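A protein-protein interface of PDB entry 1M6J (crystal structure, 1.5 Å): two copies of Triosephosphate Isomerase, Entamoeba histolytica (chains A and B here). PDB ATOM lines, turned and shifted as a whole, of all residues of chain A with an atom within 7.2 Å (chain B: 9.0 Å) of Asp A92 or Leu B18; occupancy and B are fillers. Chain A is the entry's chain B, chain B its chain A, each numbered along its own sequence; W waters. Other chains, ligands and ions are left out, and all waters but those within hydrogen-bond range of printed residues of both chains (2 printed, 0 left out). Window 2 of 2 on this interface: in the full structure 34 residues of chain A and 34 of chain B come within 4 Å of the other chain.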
ATOM      1  N   HIS A  86      22.644  15.685   5.268  1.00  0.00           N
ATOM      2  CA  HIS A  86      21.253  15.676   5.702  1.00  0.00           C
ATOM      3  C   HIS A  86      20.359  14.726   4.913  1.00  0.00           C
ATOM      4  O   HIS A  86      20.612  14.433   3.749  1.00  0.00           O
ATOM      5  CB  HIS A  86      20.694  17.104   5.596  1.00  0.00           C
ATOM      6  CG  HIS A  86      19.390  17.307   6.304  1.00  0.00           C
ATOM      7  ND1 HIS A  86      19.305  17.843   7.570  1.00  0.00           N
ATOM      8  CD2 HIS A  86      18.119  17.042   5.923  1.00  0.00           C
ATOM      9  CE1 HIS A  86      18.037  17.900   7.939  1.00  0.00           C
ATOM     10  NE2 HIS A  86      17.296  17.419   6.957  1.00  0.00           N
ATOM     11  N   VAL A  87      19.312  14.250   5.579  1.00  0.00           N
ATOM     12  CA  VAL A  87      18.316  13.373   4.975  1.00  0.00           C
ATOM     13  C   VAL A  87      17.797  14.016   3.684  1.00  0.00           C
ATOM     14  O   VAL A  87      17.632  13.351   2.663  1.00  0.00           O
ATOM     15  CB  VAL A  87      17.129  13.163   5.959  1.00  0.00           C
ATOM     16  CG1 VAL A  87      15.870  12.754   5.203  1.00  0.00           C
ATOM     17  CG2 VAL A  87      17.491  12.107   6.996  1.00  0.00           C
ATOM     18  N   GLY A  88      17.546  15.320   3.741  1.00  0.00           N
ATOM     19  CA  GLY A  88      17.037  16.040   2.589  1.00  0.00           C
ATOM     20  C   GLY A  88      17.960  16.029   1.391  1.00  0.00           C
ATOM     21  O   GLY A  88      17.507  16.114   0.251  1.00  0.00           O
ATOM     22  N   MET A  89      19.261  15.939   1.642  1.00  0.00           N
ATOM     23  CA  MET A  89      20.222  15.907   0.555  1.00  0.00           C
ATOM     24  C   MET A  89      20.118  14.565  -0.159  1.00  0.00           C
ATOM     25  O   MET A  89      20.264  14.490  -1.375  1.00  0.00           O
ATOM     26  CB  MET A  89      21.633  16.121   1.099  1.00  0.00           C
ATOM     27  CG  MET A  89      21.804  17.453   1.810  1.00  0.00           C
ATOM     28  SD  MET A  89      23.454  17.621   2.480  1.00  0.00           S
ATOM     29  CE  MET A  89      23.487  19.374   2.879  1.00  0.00           C
ATOM     30  N   LEU A  90      19.866  13.504   0.599  1.00  0.00           N
ATOM     31  CA  LEU A  90      19.726  12.184  -0.004  1.00  0.00           C
ATOM     32  C   LEU A  90      18.504  12.185  -0.917  1.00  0.00           C
ATOM     33  O   LEU A  90      18.560  11.706  -2.051  1.00  0.00           O
ATOM     34  CB  LEU A  90      19.558  11.111   1.075  1.00  0.00           C
ATOM     35  CG  LEU A  90      20.685  10.979   2.100  1.00  0.00           C
ATOM     36  CD1 LEU A  90      20.396   9.785   3.003  1.00  0.00           C
ATOM     37  CD2 LEU A  90      22.026  10.805   1.393  1.00  0.00           C
ATOM     38  N   VAL A  91      17.403  12.735  -0.421  1.00  0.00           N
ATOM     39  CA  VAL A  91      16.174  12.807  -1.203  1.00  0.00           C
ATOM     40  C   VAL A  91      16.394  13.680  -2.441  1.00  0.00           C
ATOM     41  O   VAL A  91      15.972  13.333  -3.544  1.00  0.00           O
ATOM     42  CB  VAL A  91      15.015  13.383  -0.358  1.00  0.00           C
ATOM     43  CG1 VAL A  91      13.763  13.506  -1.209  1.00  0.00           C
ATOM     44  CG2 VAL A  91      14.751  12.480   0.844  1.00  0.00           C
ATOM     45  N   ASP A  92      17.067  14.811  -2.248  1.00  0.00           N
ATOM     46  CA  ASP A  92      17.368  15.732  -3.339  1.00  0.00           C
ATOM     47  C   ASP A  92      18.176  15.012  -4.423  1.00  0.00           C
ATOM     48  O   ASP A  92      17.991  15.255  -5.619  1.00  0.00           O
ATOM     49  CB  ASP A  92      18.149  16.932  -2.783  1.00  0.00           C
ATOM     50  CG  ASP A  92      18.524  17.941  -3.850  1.00  0.00           C
ATOM     51  OD1 ASP A  92      17.616  18.445  -4.541  1.00  0.00           O
ATOM     52  OD2 ASP A  92      19.729  18.239  -3.985  1.00  0.00           O
ATOM     53  N   CYS A  93      19.059  14.113  -4.001  1.00  0.00           N
ATOM     54  CA  CYS A  93      19.891  13.362  -4.935  1.00  0.00           C
ATOM     55  C   CYS A  93      19.245  12.066  -5.422  1.00  0.00           C
ATOM     56  O   CYS A  93      19.909  11.220  -6.020  1.00  0.00           O
ATOM     57  CB  CYS A  93      21.248  13.066  -4.295  1.00  0.00           C
ATOM     58  SG  CYS A  93      22.276  14.548  -4.119  1.00  0.00           S
ATOM     59  N   GLN A  94      17.950  11.918  -5.156  1.00  0.00           N
ATOM     60  CA  GLN A  94      17.187  10.746  -5.578  1.00  0.00           C
ATOM     61  C   GLN A  94      17.676   9.407  -5.035  1.00  0.00           C
ATOM     62  O   GLN A  94      17.596   8.381  -5.713  1.00  0.00           O
ATOM     63  CB  GLN A  94      17.111  10.703  -7.107  1.00  0.00           C
ATOM     64  CG  GLN A  94      16.372  11.902  -7.689  1.00  0.00           C
ATOM     65  CD  GLN A  94      16.194  11.819  -9.190  1.00  0.00           C
ATOM     66  OE1 GLN A  94      15.586  12.699  -9.801  1.00  0.00           O
ATOM     67  NE2 GLN A  94      16.725  10.761  -9.796  1.00  0.00           N
ATOM     68  N   VAL A  95      18.184   9.427  -3.808  1.00  0.00           N
ATOM     69  CA  VAL A  95      18.644   8.215  -3.141  1.00  0.00           C
ATOM     70  C   VAL A  95      17.407   7.697  -2.408  1.00  0.00           C
ATOM     71  O   VAL A  95      16.852   8.390  -1.556  1.00  0.00           O
ATOM     72  CB  VAL A  95      19.767   8.539  -2.134  1.00  0.00           C
ATOM     73  CG1 VAL A  95      20.184   7.279  -1.391  1.00  0.00           C
ATOM     74  CG2 VAL A  95      20.962   9.140  -2.869  1.00  0.00           C
ATOM     75  N   LEU A 128      12.239   8.688   2.569  1.00  0.00           N
ATOM     76  CA  LEU A 128      13.255   7.656   2.443  1.00  0.00           C
ATOM     77  C   LEU A 128      12.783   6.327   3.003  1.00  0.00           C
ATOM     78  O   LEU A 128      11.942   6.278   3.905  1.00  0.00           O
ATOM     79  CB  LEU A 128      14.529   8.055   3.194  1.00  0.00           C
ATOM     80  CG  LEU A 128      15.316   9.253   2.668  1.00  0.00           C
ATOM     81  CD1 LEU A 128      16.495   9.546   3.588  1.00  0.00           C
ATOM     82  CD2 LEU A 128      15.804   8.955   1.265  1.00  0.00           C
ATOM     83  N   TRP B  12      30.292  25.550   3.662  1.00  0.00           N
ATOM     84  CA  TRP B  12      28.853  25.444   3.441  1.00  0.00           C
ATOM     85  C   TRP B  12      28.146  24.609   4.493  1.00  0.00           C
ATOM     86  O   TRP B  12      26.917  24.554   4.519  1.00  0.00           O
ATOM     87  CB  TRP B  12      28.557  24.833   2.071  1.00  0.00           C
ATOM     88  CG  TRP B  12      29.116  25.586   0.907  1.00  0.00           C
ATOM     89  CD1 TRP B  12      29.766  26.791   0.929  1.00  0.00           C
ATOM     90  CD2 TRP B  12      29.073  25.177  -0.463  1.00  0.00           C
ATOM     91  NE1 TRP B  12      30.130  27.155  -0.350  1.00  0.00           N
ATOM     92  CE2 TRP B  12      29.716  26.181  -1.221  1.00  0.00           C
ATOM     93  CE3 TRP B  12      28.549  24.057  -1.126  1.00  0.00           C
ATOM     94  CZ2 TRP B  12      29.854  26.098  -2.610  1.00  0.00           C
ATOM     95  CZ3 TRP B  12      28.686  23.974  -2.511  1.00  0.00           C
ATOM     96  CH2 TRP B  12      29.333  24.990  -3.235  1.00  0.00           C
ATOM     97  N   ASN B  15      24.304  22.427   4.426  1.00  0.00           N
ATOM     98  CA  ASN B  15      23.315  23.221   3.700  1.00  0.00           C
ATOM     99  C   ASN B  15      23.431  22.985   2.207  1.00  0.00           C
ATOM    100  O   ASN B  15      24.516  22.709   1.696  1.00  0.00           O
ATOM    101  CB  ASN B  15      23.550  24.720   3.927  1.00  0.00           C
ATOM    102  CG  ASN B  15      23.480  25.123   5.382  1.00  0.00           C
ATOM    103  OD1 ASN B  15      22.405  25.412   5.910  1.00  0.00           O
ATOM    104  ND2 ASN B  15      24.634  25.155   6.040  1.00  0.00           N
ATOM    105  N   GLY B  16      22.307  23.120   1.510  1.00  0.00           N
ATOM    106  CA  GLY B  16      22.322  22.990   0.068  1.00  0.00           C
ATOM    107  C   GLY B  16      21.466  21.935  -0.592  1.00  0.00           C
ATOM    108  O   GLY B  16      21.126  20.910  -0.002  1.00  0.00           O
ATOM    109  N   THR B  17      21.112  22.231  -1.838  1.00  0.00           N
ATOM    110  CA  THR B  17      20.398  21.358  -2.705  1.00  0.00           C
ATOM    111  C   THR B  17      21.084  21.449  -4.028  1.00  0.00           C
ATOM    112  O   THR B  17      21.898  22.328  -4.276  1.00  0.00           O
ATOM    113  CB  THR B  17      18.962  21.869  -2.823  1.00  0.00           C
ATOM    114  OG1 THR B  17      18.981  23.190  -3.368  1.00  0.00           O
ATOM    115  CG2 THR B  17      18.305  21.913  -1.441  1.00  0.00           C
ATOM    116  N   LEU B  18      20.829  20.527  -4.947  1.00  0.00           N
ATOM    117  CA  LEU B  18      21.494  20.577  -6.242  1.00  0.00           C
ATOM    118  C   LEU B  18      21.233  21.924  -6.908  1.00  0.00           C
ATOM    119  O   LEU B  18      22.127  22.511  -7.514  1.00  0.00           O
ATOM    120  CB  LEU B  18      20.992  19.443  -7.140  1.00  0.00           C
ATOM    121  CG  LEU B  18      21.419  18.028  -6.734  1.00  0.00           C
ATOM    122  CD1 LEU B  18      20.635  17.001  -7.536  1.00  0.00           C
ATOM    123  CD2 LEU B  18      22.915  17.858  -6.965  1.00  0.00           C
ATOM    124  N   ALA B  19      20.007  22.419  -6.781  1.00  0.00           N
ATOM    125  CA  ALA B  19      19.645  23.692  -7.387  1.00  0.00           C
ATOM    126  C   ALA B  19      20.361  24.874  -6.740  1.00  0.00           C
ATOM    127  O   ALA B  19      20.902  25.729  -7.439  1.00  0.00           O
ATOM    128  CB  ALA B  19      18.127  23.894  -7.318  1.00  0.00           C
ATOM    129  N   SER B  20      20.379  24.924  -5.411  1.00  0.00           N
ATOM    130  CA  SER B  20      21.026  26.047  -4.735  1.00  0.00           C
ATOM    131  C   SER B  20      22.538  26.014  -4.918  1.00  0.00           C
ATOM    132  O   SER B  20      23.183  27.058  -5.021  1.00  0.00           O
ATOM    133  CB  SER B  20      20.676  26.062  -3.242  1.00  0.00           C
ATOM    134  OG  SER B  20      21.418  25.104  -2.508  1.00  0.00           O
ATOM    135  N   ILE B  21      23.100  24.812  -4.972  1.00  0.00           N
ATOM    136  CA  ILE B  21      24.536  24.659  -5.140  1.00  0.00           C
ATOM    137  C   ILE B  21      24.994  25.023  -6.553  1.00  0.00           C
ATOM    138  O   ILE B  21      26.081  25.569  -6.733  1.00  0.00           O
ATOM    139  CB  ILE B  21      24.965  23.224  -4.759  1.00  0.00           C
ATOM    140  CG1 ILE B  21      24.850  23.069  -3.238  1.00  0.00           C
ATOM    141  CG2 ILE B  21      26.380  22.934  -5.240  1.00  0.00           C
ATOM    142  CD1 ILE B  21      25.137  21.677  -2.717  1.00  0.00           C
ATOM    143  N   GLU B  22      24.168  24.741  -7.556  1.00  0.00           N
ATOM    144  CA  GLU B  22      24.546  25.093  -8.917  1.00  0.00           C
ATOM    145  C   GLU B  22      24.599  26.615  -9.020  1.00  0.00           C
ATOM    146  O   GLU B  22      25.538  27.176  -9.583  1.00  0.00           O
ATOM    147  CB  GLU B  22      23.549  24.529  -9.935  1.00  0.00           C
ATOM    148  CG  GLU B  22      24.036  24.675 -11.373  1.00  0.00           C
ATOM    149  CD  GLU B  22      23.184  23.920 -12.369  1.00  0.00           C
ATOM    150  OE1 GLU B  22      22.929  22.718 -12.141  1.00  0.00           O
ATOM    151  OE2 GLU B  22      22.780  24.523 -13.386  1.00  0.00           O
ATOM    152  N   THR B  23      23.599  27.283  -8.456  1.00  0.00           N
ATOM    153  CA  THR B  23      23.556  28.741  -8.492  1.00  0.00           C
ATOM    154  C   THR B  23      24.718  29.337  -7.699  1.00  0.00           C
ATOM    155  O   THR B  23      25.378  30.271  -8.154  1.00  0.00           O
ATOM    156  CB  THR B  23      22.231  29.276  -7.916  1.00  0.00           C
ATOM    157  OG1 THR B  23      21.138  28.781  -8.699  1.00  0.00           O
ATOM    158  CG2 THR B  23      22.213  30.800  -7.938  1.00  0.00           C
ATOM    159  N   LEU B  24      24.971  28.784  -6.517  1.00  0.00           N
ATOM    160  CA  LEU B  24      26.050  29.271  -5.665  1.00  0.00           C
ATOM    161  C   LEU B  24      27.429  29.058  -6.282  1.00  0.00           C
ATOM    162  O   LEU B  24      28.239  29.980  -6.331  1.00  0.00           O
ATOM    163  CB  LEU B  24      25.991  28.589  -4.290  1.00  0.00           C
ATOM    164  CG  LEU B  24      27.091  28.929  -3.276  1.00  0.00           C
ATOM    165  CD1 LEU B  24      27.122  30.432  -3.009  1.00  0.00           C
ATOM    166  CD2 LEU B  24      26.845  28.165  -1.983  1.00  0.00           C
ATOM    167  N   THR B  25      27.692  27.844  -6.756  1.00  0.00           N
ATOM    168  CA  THR B  25      28.984  27.529  -7.350  1.00  0.00           C
ATOM    169  C   THR B  25      29.281  28.416  -8.556  1.00  0.00           C
ATOM    170  O   THR B  25      30.394  28.915  -8.706  1.00  0.00           O
ATOM    171  CB  THR B  25      29.052  26.042  -7.756  1.00  0.00           C
ATOM    172  OG1 THR B  25      28.807  25.231  -6.599  1.00  0.00           O
ATOM    173  CG2 THR B  25      30.429  25.692  -8.312  1.00  0.00           C
ATOM    174  N   LYS B  26      28.288  28.622  -9.413  1.00  0.00           N
ATOM    175  CA  LYS B  26      28.495  29.474 -10.577  1.00  0.00           C
ATOM    176  C   LYS B  26      28.768  30.911 -10.136  1.00  0.00           C
ATOM    177  O   LYS B  26      29.603  31.597 -10.722  1.00  0.00           O
ATOM    178  CB  LYS B  26      27.281  29.422 -11.507  1.00  0.00           C
ATOM    179  CG  LYS B  26      27.180  28.121 -12.289  1.00  0.00           C
ATOM    180  CD  LYS B  26      25.933  28.073 -13.153  1.00  0.00           C
ATOM    181  CE  LYS B  26      25.875  26.774 -13.946  1.00  0.00           C
ATOM    182  NZ  LYS B  26      24.617  26.651 -14.734  1.00  0.00           N
ATOM    183  N   ILE B  49      28.193  14.320  -0.531  1.00  0.00           N
ATOM    184  CA  ILE B  49      27.369  13.917  -1.663  1.00  0.00           C
ATOM    185  C   ILE B  49      27.300  14.914  -2.816  1.00  0.00           C
ATOM    186  O   ILE B  49      26.974  14.538  -3.945  1.00  0.00           O
ATOM    187  CB  ILE B  49      25.938  13.562  -1.176  1.00  0.00           C
ATOM    188  CG1 ILE B  49      25.224  12.702  -2.222  1.00  0.00           C
ATOM    189  CG2 ILE B  49      25.155  14.838  -0.879  1.00  0.00           C
ATOM    190  CD1 ILE B  49      23.928  12.076  -1.723  1.00  0.00           C
ATOM    191  N   TYR B  50      27.624  16.175  -2.547  1.00  0.00           N
ATOM    192  CA  TYR B  50      27.576  17.195  -3.592  1.00  0.00           C
ATOM    193  C   TYR B  50      28.939  17.524  -4.186  1.00  0.00           C
ATOM    194  O   TYR B  50      29.038  18.357  -5.080  1.00  0.00           O
ATOM    195  CB  TYR B  50      26.938  18.484  -3.058  1.00  0.00           C
ATOM    196  CG  TYR B  50      25.466  18.360  -2.751  1.00  0.00           C
ATOM    197  CD1 TYR B  50      24.978  18.638  -1.475  1.00  0.00           C
ATOM    198  CD2 TYR B  50      24.556  17.973  -3.737  1.00  0.00           C
ATOM    199  CE1 TYR B  50      23.622  18.534  -1.185  1.00  0.00           C
ATOM    200  CE2 TYR B  50      23.192  17.865  -3.456  1.00  0.00           C
ATOM    201  CZ  TYR B  50      22.735  18.147  -2.177  1.00  0.00           C
ATOM    202  OH  TYR B  50      21.396  18.048  -1.887  1.00  0.00           O
ATOM    203  N   ILE B  51      29.991  16.876  -3.699  1.00  0.00           N
ATOM    204  CA  ILE B  51      31.321  17.157  -4.221  1.00  0.00           C
ATOM    205  C   ILE B  51      31.425  16.883  -5.720  1.00  0.00           C
ATOM    206  O   ILE B  51      31.958  17.702  -6.461  1.00  0.00           O
ATOM    207  CB  ILE B  51      32.403  16.378  -3.433  1.00  0.00           C
ATOM    208  CG1 ILE B  51      32.594  17.051  -2.066  1.00  0.00           C
ATOM    209  CG2 ILE B  51      33.719  16.344  -4.215  1.00  0.00           C
ATOM    210  CD1 ILE B  51      33.517  16.313  -1.107  1.00  0.00           C
ATOM    211  N   PRO B  52      30.908  15.737  -6.191  1.00  0.00           N
ATOM    212  CA  PRO B  52      31.008  15.487  -7.631  1.00  0.00           C
ATOM    213  C   PRO B  52      30.303  16.570  -8.453  1.00  0.00           C
ATOM    214  O   PRO B  52      30.823  17.015  -9.477  1.00  0.00           O
ATOM    215  CB  PRO B  52      30.354  14.114  -7.788  1.00  0.00           C
ATOM    216  CG  PRO B  52      30.697  13.444  -6.493  1.00  0.00           C
ATOM    217  CD  PRO B  52      30.402  14.544  -5.490  1.00  0.00           C
ATOM    218  N   LYS B  53      29.125  16.994  -8.002  1.00  0.00           N
ATOM    219  CA  LYS B  53      28.360  18.021  -8.703  1.00  0.00           C
ATOM    220  C   LYS B  53      29.128  19.334  -8.768  1.00  0.00           C
ATOM    221  O   LYS B  53      29.221  19.958  -9.825  1.00  0.00           O
ATOM    222  CB  LYS B  53      27.009  18.240  -8.010  1.00  0.00           C
ATOM    223  CG  LYS B  53      26.156  19.347  -8.620  1.00  0.00           C
ATOM    224  CD  LYS B  53      25.816  19.065 -10.074  1.00  0.00           C
ATOM    225  CE  LYS B  53      24.943  20.164 -10.654  1.00  0.00           C
ATOM    226  NZ  LYS B  53      24.603  19.897 -12.079  1.00  0.00           N
ATOM    227  N   VAL B  54      29.681  19.755  -7.636  1.00  0.00           N
ATOM    228  CA  VAL B  54      30.439  20.997  -7.600  1.00  0.00           C
ATOM    229  C   VAL B  54      31.632  20.909  -8.541  1.00  0.00           C
ATOM    230  O   VAL B  54      31.942  21.864  -9.249  1.00  0.00           O
ATOM    231  CB  VAL B  54      30.930  21.307  -6.170  1.00  0.00           C
ATOM    232  CG1 VAL B  54      31.887  22.500  -6.181  1.00  0.00           C
ATOM    233  CG2 VAL B  54      29.732  21.609  -5.277  1.00  0.00           C
ATOM    234  N   GLN B  56      31.898  19.103 -11.224  1.00  0.00           N
ATOM    235  CA  GLN B  56      31.378  19.154 -12.584  1.00  0.00           C
ATOM    236  C   GLN B  56      31.062  20.590 -12.988  1.00  0.00           C
ATOM    237  O   GLN B  56      31.403  21.024 -14.088  1.00  0.00           O
ATOM    238  CB  GLN B  56      30.113  18.299 -12.684  1.00  0.00           C
ATOM    239  CG  GLN B  56      29.506  18.233 -14.075  1.00  0.00           C
ATOM    240  CD  GLN B  56      28.220  17.431 -14.100  1.00  0.00           C
ATOM    241  OE1 GLN B  56      28.193  16.270 -13.694  1.00  0.00           O
ATOM    242  NE2 GLN B  56      27.147  18.048 -14.577  1.00  0.00           N
ATOM    243  N   ILE B  57      30.411  21.323 -12.090  1.00  0.00           N
ATOM    244  CA  ILE B  57      30.044  22.710 -12.356  1.00  0.00           C
ATOM    245  C   ILE B  57      31.285  23.568 -12.579  1.00  0.00           C
ATOM    246  O   ILE B  57      31.373  24.301 -13.565  1.00  0.00           O
ATOM    247  CB  ILE B  57      29.218  23.306 -11.188  1.00  0.00           C
ATOM    248  CG1 ILE B  57      27.903  22.536 -11.039  1.00  0.00           C
ATOM    249  CG2 ILE B  57      28.928  24.781 -11.447  1.00  0.00           C
ATOM    250  CD1 ILE B  57      27.095  22.928  -9.819  1.00  0.00           C
HETATM  251  O   HOH W   1      18.872  19.233   0.580  1.00  0.00           O
HETATM  252  O   HOH W   2      17.763  20.596  -6.156  1.00  0.00           O
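OH of Tyr B50 is in hydrogen-bond range of OD2 of Asp A92, at 2.7 Å.
OD2 of Asp A92 is in hydrogen-bond range of N of Leu B18, 2.7 Å away.
O of Trp B12 is in hydrogen-bond range of ND2 of Asn B15, at 2.8 Å.
N of Thr B17 sits at hydrogen-bond distance from OG of Ser B20, 3.0 Å away.
The side-chain sulfur (SD) of Met A89 lies within hydrogen-bond range of the backbone NH (N) of His A86 (3.5 Å).
The backbone carbonyl oxygen (O) of Gly B16 lies within hydrogen-bond range of the side-chain hydroxyl (OH) of Tyr B50.
The backbone carbonyl oxygen (O) of Met A89 lies close to the side-chain sulfur (SG) of Cys A93, 3.4 Å away.
The backbone NH (N) of Val A95 is in hydrogen-bond range of the backbone carbonyl oxygen (O) of Leu A90 (2.9 Å).
Met A89 touches Asn B15 (CE to N, 3.5 Å).
O of Gly B16 touches CG of Met A89, at 3.96 Å.
OH of Tyr B50 touches CA of Met A89, 3.5 Å away.
Ile B49 touches Leu A90 (CD1 to CD2, 3.9 Å).
OD2 of Asp A92 touches CA of Thr B17, at 3.4 Å.
Ile B49 touches Cys A93 (CD1 to SG, 3.8 Å).
Cys A93 touches Tyr B50 (SG to CE2, 3.5 Å).
Asp A92 touches just these residues of chain B: Thr B17, Leu B18 and Tyr B50.
Leu B18 touches just one residue of chain A: Asp A92 (2.7 Å).
No residue of chain B comes within 4 Å of Val A91.
Of the printed residues of chain B, Cys A93 touches Ile B49 (3.8 Å) and Tyr B50 (3.5 Å).
Printed residues of chain A within 4 Å of Thr B17: Asp A92 (3.4 Å).
Printed residues of chain B within 4 Å of Met A89: Asn B15 (3.5 Å), Gly B16 (3.96 Å) and Tyr B50 (3.5 Å).
Hydrophobic or aromatic side chains of chain A within 4 Å of the printed part of chain B: Met A89 and Leu A90.
Along chain A the printed residues that touch a printed residue of chain B span positions 89 to 93.
Of the 21 printed residues of chain B, 6 touch a printed residue of chain A.
Printed residues of chain B that touch a printed residue of chain A: Asn B15, Gly B16, Thr B17, Leu B18, Ile B49 and Tyr B50.
Hydrophobic or aromatic side chains of chain B within 4 Å of the printed part of chain A: Leu B18, Ile B49 and Tyr B50.
Among the printed residues, 9 pairs touch across the chains.
No position is printed for both chains.
Of the 9 pairs that touch across the chains among the printed residues, none has its exchanged pair printed and touching as well.
Water W2 lies within hydrogen-bond range of OD1 of Asp A92 (2.7 Å), N of Ala B19 (3.0 Å) and N of Leu B18 (3.3 Å).
Water W1 lies within hydrogen-bond range of O of Gly B16 (2.9 Å), O of Gly A88 (3.4 Å) and N of Met A89 (3.5 Å).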
